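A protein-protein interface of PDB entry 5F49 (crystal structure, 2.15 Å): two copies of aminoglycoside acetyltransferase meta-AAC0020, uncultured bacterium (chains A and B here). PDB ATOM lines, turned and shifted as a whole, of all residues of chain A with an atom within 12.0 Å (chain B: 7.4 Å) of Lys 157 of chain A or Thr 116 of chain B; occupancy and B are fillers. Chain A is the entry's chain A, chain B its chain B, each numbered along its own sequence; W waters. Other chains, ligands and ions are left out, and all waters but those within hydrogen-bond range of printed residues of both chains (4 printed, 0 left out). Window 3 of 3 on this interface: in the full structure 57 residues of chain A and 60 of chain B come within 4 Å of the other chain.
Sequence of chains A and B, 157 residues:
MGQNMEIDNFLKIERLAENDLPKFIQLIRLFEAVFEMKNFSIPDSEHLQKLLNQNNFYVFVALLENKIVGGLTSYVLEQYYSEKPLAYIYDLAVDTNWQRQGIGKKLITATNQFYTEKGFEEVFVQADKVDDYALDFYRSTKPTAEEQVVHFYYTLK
Water W3 lies within hydrogen-bond range of the backbone carbonyl oxygen of Leu 156 of chain A (2.4 Å) and the backbone carbonyl oxygen of Glu 121 of chain B (2.7 Å).
Water W4 bridges the chain-end carboxylate (O) of Lys 157 of chain A (2.5 Å) and the backbone carbonyl oxygen (O) of Thr 116 of chain B (2.9 Å).
Water W2 bridges the side-chain hydroxyl of Thr 116 of chain B (2.9 Å) and the backbone NH of Lys 157 of chain A (3.0 Å).
Water W1 lies within hydrogen-bond range of the backbone carbonyl oxygen (O) of Phe 120 of chain B (2.9 Å) and the chain-end carboxylate (O) of Lys 157 of chain A (3.0 Å).
OG1 of Thr 116 of chain B is in hydrogen-bond range of O of Asn 112 of chain B (2.7 Å).
The backbone NH (N) of Phe 120 of chain B is in hydrogen-bond range of the backbone carbonyl oxygen (O) of Tyr 115 of chain B (3.0 Å).
Hydrophobic or aromatic side chains of chain B within 4 Å of the printed part of chain A: Tyr 115, Phe 120 and Val 123.
Of the 5 printed residues of chain A, 5 touch a printed residue of chain B.
Among the printed residues, 10 pairs touch across the chains.
Among the printed residues, no Asp or Glu carboxylate lies within 4 Å of a Lys or Arg side-chain nitrogen of the other chain.
Of the printed residues of chain B, Tyr 154 of chain A touches Asn 112 (3.2 Å) and Val 123 (2.7 Å).
Printed residues of chain B within 4 Å of Leu 156 of chain A: Tyr 115, Thr 116, Phe 120, Glu 121 and Val 123.
Of chain B, only Thr 116 (3.8 Å) comes within 4 Å of Lys 157 of chain A.
Thr 109 of chain B touches none of the printed residues of chain A.
Of chain A, only Tyr 154 (3.2 Å) comes within 4 Å of Asn 112 of chain B.
No residue of chain A comes within 4 Å of Gln 113 of chain B.
No residue of chain A comes within 4 Å of Phe 114 of chain B.
Printed residues of chain A within 4 Å of Tyr 115 of chain B: Leu 156.
Glu 117 of chain B touches none of the printed residues of chain A.
No residue of chain A comes within 4 Å of Lys 118 of chain B.
No residue of chain A comes within 4 Å of Gly 119 of chain B.
Phe 120 of chain B touches one residue of chain A.
Of the printed residues of chain A, Val 123 of chain B touches Tyr 153, Tyr 154 and Leu 156.
No position is printed for both chains.
Of the 10 pairs that touch across the chains among the printed residues, none has its exchanged pair printed and touching as well.
Among the printed residues, merely in contact across the chains: Tyr 154 of chain A with Asn 112 of chain B (3.2 Å), Tyr 153 of chain A with Val 123 of chain B (3.3 Å), Leu 156 of chain A with Phe 120 of chain B (3.6 Å), Leu 156 of chain A with Thr 116 of chain B (3.7 Å), Leu 156 of chain A with Tyr 115 of chain B (3.7 Å), Lys 157 of chain A with Thr 116 of chain B (3.8 Å), Thr 155 of chain A with Glu 121 of chain B (3.98 Å) and Leu 156 of chain A with Val 123 of chain B (3.99 Å).
O of Val 123 of chain B is in hydrogen-bond range of N of Tyr 154 of chain A, at 2.7 Å.
The backbone carbonyl oxygen (O) of Glu 121 of chain B is in hydrogen-bond range of the backbone NH (N) of Leu 156 of chain A (3.1 Å).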
ATOM      1  N   TYR A 153      -6.993  31.872  25.343  1.00  0.00           N
ATOM      2  CA  TYR A 153      -5.999  30.840  25.595  1.00  0.00           C
ATOM      3  C   TYR A 153      -5.116  30.542  24.393  1.00  0.00           C
ATOM      4  O   TYR A 153      -5.475  30.807  23.239  1.00  0.00           O
ATOM      5  CB  TYR A 153      -6.655  29.544  26.116  1.00  0.00           C
ATOM      6  CG  TYR A 153      -7.647  28.833  25.212  1.00  0.00           C
ATOM      7  CD1 TYR A 153      -7.222  27.889  24.278  1.00  0.00           C
ATOM      8  CD2 TYR A 153      -9.015  29.050  25.344  1.00  0.00           C
ATOM      9  CE1 TYR A 153      -8.131  27.215  23.467  1.00  0.00           C
ATOM     10  CE2 TYR A 153      -9.931  28.382  24.539  1.00  0.00           C
ATOM     11  CZ  TYR A 153      -9.482  27.467  23.603  1.00  0.00           C
ATOM     12  OH  TYR A 153     -10.393  26.806  22.806  1.00  0.00           O
ATOM     13  N   TYR A 154      -3.937  30.014  24.701  1.00  0.00           N
ATOM     14  CA  TYR A 154      -2.958  29.617  23.705  1.00  0.00           C
ATOM     15  C   TYR A 154      -2.729  28.116  23.826  1.00  0.00           C
ATOM     16  O   TYR A 154      -2.120  27.648  24.794  1.00  0.00           O
ATOM     17  CB  TYR A 154      -1.636  30.374  23.893  1.00  0.00           C
ATOM     18  CG  TYR A 154      -1.778  31.883  24.027  1.00  0.00           C
ATOM     19  CD1 TYR A 154      -2.090  32.464  25.251  1.00  0.00           C
ATOM     20  CD2 TYR A 154      -1.589  32.721  22.939  1.00  0.00           C
ATOM     21  CE1 TYR A 154      -2.224  33.838  25.383  1.00  0.00           C
ATOM     22  CE2 TYR A 154      -1.719  34.101  23.062  1.00  0.00           C
ATOM     23  CZ  TYR A 154      -2.036  34.649  24.288  1.00  0.00           C
ATOM     24  OH  TYR A 154      -2.166  36.012  24.431  1.00  0.00           O
ATOM     25  N   THR A 155      -3.226  27.356  22.859  1.00  0.00           N
ATOM     26  CA  THR A 155      -2.949  25.927  22.823  1.00  0.00           C
ATOM     27  C   THR A 155      -1.529  25.709  22.315  1.00  0.00           C
ATOM     28  O   THR A 155      -1.209  26.084  21.191  1.00  0.00           O
ATOM     29  CB  THR A 155      -3.950  25.172  21.934  1.00  0.00           C
ATOM     30  OG1 THR A 155      -5.285  25.467  22.365  1.00  0.00           O
ATOM     31  CG2 THR A 155      -3.710  23.667  22.026  1.00  0.00           C
ATOM     32  N   LEU A 156      -0.682  25.107  23.146  1.00  0.00           N
ATOM     33  CA  LEU A 156       0.736  24.976  22.824  1.00  0.00           C
ATOM     34  C   LEU A 156       1.019  23.727  21.992  1.00  0.00           C
ATOM     35  O   LEU A 156       0.279  22.748  22.051  1.00  0.00           O
ATOM     36  CB  LEU A 156       1.574  24.953  24.107  1.00  0.00           C
ATOM     37  CG  LEU A 156       1.285  26.048  25.142  1.00  0.00           C
ATOM     38  CD1 LEU A 156       2.245  25.942  26.309  1.00  0.00           C
ATOM     39  CD2 LEU A 156       1.347  27.436  24.519  1.00  0.00           C
ATOM     40  N   LYS A 157       2.090  23.772  21.207  1.00  0.00           N
ATOM     41  CA  LYS A 157       2.513  22.606  20.446  1.00  0.00           C
ATOM     42  C   LYS A 157       3.371  21.693  21.320  1.00  0.00           C
ATOM     43  O   LYS A 157       3.886  22.116  22.356  1.00  0.00           O
ATOM     44  CB  LYS A 157       3.285  23.024  19.194  1.00  0.00           C
ATOM     45  CG  LYS A 157       2.442  23.730  18.154  1.00  0.00           C
ATOM     46  CD  LYS A 157       3.263  24.081  16.927  1.00  0.00           C
ATOM     47  CE  LYS A 157       2.405  24.740  15.856  1.00  0.00           C
ATOM     48  NZ  LYS A 157       3.203  25.118  14.653  1.00  0.00           N
ATOM     49  OXT LYS A 157       3.564  20.513  21.020  1.00  0.00           O
ATOM     50  N   LYS B  84      -0.113  17.127  31.467  1.00  0.00           N
ATOM     51  CA  LYS B  84       0.411  18.379  30.927  1.00  0.00           C
ATOM     52  C   LYS B  84      -0.255  19.552  31.644  1.00  0.00           C
ATOM     53  O   LYS B  84      -1.464  19.743  31.540  1.00  0.00           O
ATOM     54  CB  LYS B  84       0.185  18.468  29.414  1.00  0.00           C
ATOM     55  CG  LYS B  84       0.938  17.419  28.602  1.00  0.00           C
ATOM     56  CD  LYS B  84       0.703  17.598  27.107  1.00  0.00           C
ATOM     57  CE  LYS B  84       1.482  16.575  26.290  1.00  0.00           C
ATOM     58  NZ  LYS B  84       1.242  16.707  24.821  1.00  0.00           N
ATOM     59  N   THR B 109       5.044  36.320  24.029  1.00  0.00           N
ATOM     60  CA  THR B 109       5.754  35.361  23.193  1.00  0.00           C
ATOM     61  C   THR B 109       6.734  34.537  24.028  1.00  0.00           C
ATOM     62  O   THR B 109       6.698  33.304  23.999  1.00  0.00           O
ATOM     63  CB  THR B 109       6.521  36.059  22.045  1.00  0.00           C
ATOM     64  OG1 THR B 109       5.585  36.626  21.120  1.00  0.00           O
ATOM     65  CG2 THR B 109       7.407  35.064  21.306  1.00  0.00           C
ATOM     66  N   ALA B 110       7.594  35.227  24.775  1.00  0.00           N
ATOM     67  CA  ALA B 110       8.573  34.573  25.635  1.00  0.00           C
ATOM     68  C   ALA B 110       7.902  33.648  26.654  1.00  0.00           C
ATOM     69  O   ALA B 110       8.396  32.557  26.933  1.00  0.00           O
ATOM     70  CB  ALA B 110       9.428  35.611  26.349  1.00  0.00           C
ATOM     71  N   THR B 111       6.771  34.088  27.196  1.00  0.00           N
ATOM     72  CA  THR B 111       6.056  33.323  28.216  1.00  0.00           C
ATOM     73  C   THR B 111       5.513  32.015  27.645  1.00  0.00           C
ATOM     74  O   THR B 111       5.695  30.940  28.225  1.00  0.00           O
ATOM     75  CB  THR B 111       4.891  34.138  28.823  1.00  0.00           C
ATOM     76  OG1 THR B 111       5.407  35.296  29.495  1.00  0.00           O
ATOM     77  CG2 THR B 111       4.120  33.305  29.814  1.00  0.00           C
ATOM     78  N   ASN B 112       4.841  32.109  26.505  1.00  0.00           N
ATOM     79  CA  ASN B 112       4.311  30.917  25.853  1.00  0.00           C
ATOM     80  C   ASN B 112       5.412  29.995  25.362  1.00  0.00           C
ATOM     81  O   ASN B 112       5.245  28.775  25.351  1.00  0.00           O
ATOM     82  CB  ASN B 112       3.399  31.307  24.690  1.00  0.00           C
ATOM     83  CG  ASN B 112       2.102  31.918  25.165  1.00  0.00           C
ATOM     84  OD1 ASN B 112       1.748  31.796  26.339  1.00  0.00           O
ATOM     85  ND2 ASN B 112       1.386  32.581  24.265  1.00  0.00           N
ATOM     86  N   GLN B 113       6.529  30.581  24.942  1.00  0.00           N
ATOM     87  CA  GLN B 113       7.675  29.796  24.513  1.00  0.00           C
ATOM     88  C   GLN B 113       8.226  28.985  25.679  1.00  0.00           C
ATOM     89  O   GLN B 113       8.569  27.814  25.522  1.00  0.00           O
ATOM     90  CB  GLN B 113       8.762  30.702  23.926  1.00  0.00           C
ATOM     91  CG  GLN B 113      10.096  30.011  23.664  1.00  0.00           C
ATOM     92  CD  GLN B 113       9.995  28.839  22.695  1.00  0.00           C
ATOM     93  OE1 GLN B 113       9.041  28.729  21.919  1.00  0.00           O
ATOM     94  NE2 GLN B 113      10.989  27.958  22.737  1.00  0.00           N
ATOM     95  N   PHE B 114       8.301  29.615  26.848  1.00  0.00           N
ATOM     96  CA  PHE B 114       8.809  28.957  28.045  1.00  0.00           C
ATOM     97  C   PHE B 114       7.927  27.785  28.450  1.00  0.00           C
ATOM     98  O   PHE B 114       8.421  26.703  28.753  1.00  0.00           O
ATOM     99  CB  PHE B 114       8.919  29.953  29.207  1.00  0.00           C
ATOM    100  CG  PHE B 114       9.167  29.304  30.545  1.00  0.00           C
ATOM    101  CD1 PHE B 114      10.430  28.841  30.886  1.00  0.00           C
ATOM    102  CD2 PHE B 114       8.135  29.155  31.461  1.00  0.00           C
ATOM    103  CE1 PHE B 114      10.658  28.239  32.117  1.00  0.00           C
ATOM    104  CE2 PHE B 114       8.355  28.555  32.690  1.00  0.00           C
ATOM    105  CZ  PHE B 114       9.619  28.100  33.019  1.00  0.00           C
ATOM    106  N   TYR B 115       6.618  27.998  28.459  1.00  0.00           N
ATOM    107  CA  TYR B 115       5.716  26.948  28.895  1.00  0.00           C
ATOM    108  C   TYR B 115       5.623  25.863  27.816  1.00  0.00           C
ATOM    109  O   TYR B 115       5.330  24.700  28.112  1.00  0.00           O
ATOM    110  CB  TYR B 115       4.339  27.530  29.240  1.00  0.00           C
ATOM    111  CG  TYR B 115       4.314  28.229  30.592  1.00  0.00           C
ATOM    112  CD1 TYR B 115       4.597  27.522  31.757  1.00  0.00           C
ATOM    113  CD2 TYR B 115       4.015  29.588  30.707  1.00  0.00           C
ATOM    114  CE1 TYR B 115       4.575  28.135  32.990  1.00  0.00           C
ATOM    115  CE2 TYR B 115       4.004  30.218  31.952  1.00  0.00           C
ATOM    116  CZ  TYR B 115       4.279  29.479  33.086  1.00  0.00           C
ATOM    117  OH  TYR B 115       4.267  30.063  34.334  1.00  0.00           O
ATOM    118  N   THR B 116       5.910  26.239  26.571  1.00  0.00           N
ATOM    119  CA  THR B 116       5.977  25.262  25.486  1.00  0.00           C
ATOM    120  C   THR B 116       7.137  24.294  25.687  1.00  0.00           C
ATOM    121  O   THR B 116       6.978  23.083  25.535  1.00  0.00           O
ATOM    122  CB  THR B 116       6.129  25.937  24.111  1.00  0.00           C
ATOM    123  OG1 THR B 116       4.917  26.623  23.783  1.00  0.00           O
ATOM    124  CG2 THR B 116       6.434  24.896  23.024  1.00  0.00           C
ATOM    125  N   GLU B 117       8.303  24.834  26.032  1.00  0.00           N
ATOM    126  CA  GLU B 117       9.486  24.015  26.292  1.00  0.00           C
ATOM    127  C   GLU B 117       9.256  23.079  27.465  1.00  0.00           C
ATOM    128  O   GLU B 117       9.892  22.033  27.573  1.00  0.00           O
ATOM    129  CB  GLU B 117      10.705  24.890  26.582  1.00  0.00           C
ATOM    130  CG  GLU B 117      11.072  25.865  25.486  1.00  0.00           C
ATOM    131  CD  GLU B 117      12.132  26.859  25.928  1.00  0.00           C
ATOM    132  OE1 GLU B 117      12.377  26.963  27.150  1.00  0.00           O
ATOM    133  OE2 GLU B 117      12.720  27.536  25.056  1.00  0.00           O
ATOM    134  N   LYS B 118       8.349  23.474  28.348  1.00  0.00           N
ATOM    135  CA  LYS B 118       8.088  22.734  29.572  1.00  0.00           C
ATOM    136  C   LYS B 118       6.989  21.700  29.352  1.00  0.00           C
ATOM    137  O   LYS B 118       6.647  20.947  30.260  1.00  0.00           O
ATOM    138  CB  LYS B 118       7.707  23.696  30.703  1.00  0.00           C
ATOM    139  CG  LYS B 118       8.896  24.260  31.489  1.00  0.00           C
ATOM    140  CD  LYS B 118      10.140  24.408  30.616  1.00  0.00           C
ATOM    141  CE  LYS B 118      11.409  24.609  31.426  1.00  0.00           C
ATOM    142  NZ  LYS B 118      12.616  24.425  30.563  1.00  0.00           N
ATOM    143  N   GLY B 119       6.444  21.670  28.141  1.00  0.00           N
ATOM    144  CA  GLY B 119       5.448  20.682  27.771  1.00  0.00           C
ATOM    145  C   GLY B 119       4.059  20.973  28.317  1.00  0.00           C
ATOM    146  O   GLY B 119       3.254  20.063  28.476  1.00  0.00           O
ATOM    147  N   PHE B 120       3.763  22.234  28.601  1.00  0.00           N
ATOM    148  CA  PHE B 120       2.430  22.569  29.084  1.00  0.00           C
ATOM    149  C   PHE B 120       1.416  22.376  27.971  1.00  0.00           C
ATOM    150  O   PHE B 120       1.759  22.444  26.794  1.00  0.00           O
ATOM    151  CB  PHE B 120       2.378  23.999  29.605  1.00  0.00           C
ATOM    152  CG  PHE B 120       2.901  24.153  30.998  1.00  0.00           C
ATOM    153  CD1 PHE B 120       4.087  23.541  31.381  1.00  0.00           C
ATOM    154  CD2 PHE B 120       2.214  24.922  31.925  1.00  0.00           C
ATOM    155  CE1 PHE B 120       4.574  23.689  32.662  1.00  0.00           C
ATOM    156  CE2 PHE B 120       2.694  25.079  33.205  1.00  0.00           C
ATOM    157  CZ  PHE B 120       3.877  24.463  33.579  1.00  0.00           C
ATOM    158  N   GLU B 121       0.170  22.116  28.347  1.00  0.00           N
ATOM    159  CA  GLU B 121      -0.891  21.968  27.371  1.00  0.00           C
ATOM    160  C   GLU B 121      -1.351  23.325  26.846  1.00  0.00           C
ATOM    161  O   GLU B 121      -1.593  23.481  25.652  1.00  0.00           O
ATOM    162  CB  GLU B 121      -2.082  21.216  27.975  1.00  0.00           C
ATOM    163  CG  GLU B 121      -3.295  21.187  27.068  1.00  0.00           C
ATOM    164  CD  GLU B 121      -4.507  20.553  27.716  1.00  0.00           C
ATOM    165  OE1 GLU B 121      -5.635  20.900  27.315  1.00  0.00           O
ATOM    166  OE2 GLU B 121      -4.337  19.709  28.619  1.00  0.00           O
ATOM    167  N   VAL B 123      -1.700  27.896  27.868  1.00  0.00           N
ATOM    168  CA  VAL B 123      -1.576  29.109  28.672  1.00  0.00           C
ATOM    169  C   VAL B 123      -2.838  29.954  28.493  1.00  0.00           C
ATOM    170  O   VAL B 123      -3.281  30.154  27.364  1.00  0.00           O
ATOM    171  CB  VAL B 123      -0.339  29.952  28.266  1.00  0.00           C
ATOM    172  CG1 VAL B 123      -0.219  31.179  29.149  1.00  0.00           C
ATOM    173  CG2 VAL B 123       0.937  29.117  28.343  1.00  0.00           C
HETATM  174  O   HOH W   1       3.111  20.729  24.921  1.00  0.00           O
HETATM  175  O   HOH W   2       3.558  26.405  21.285  1.00  0.00           O
HETATM  176  O   HOH W   3      -1.315  21.756  23.607  1.00  0.00           O
HETATM  177  O   HOH W   4       5.973  21.274  23.531  1.00  0.00           O
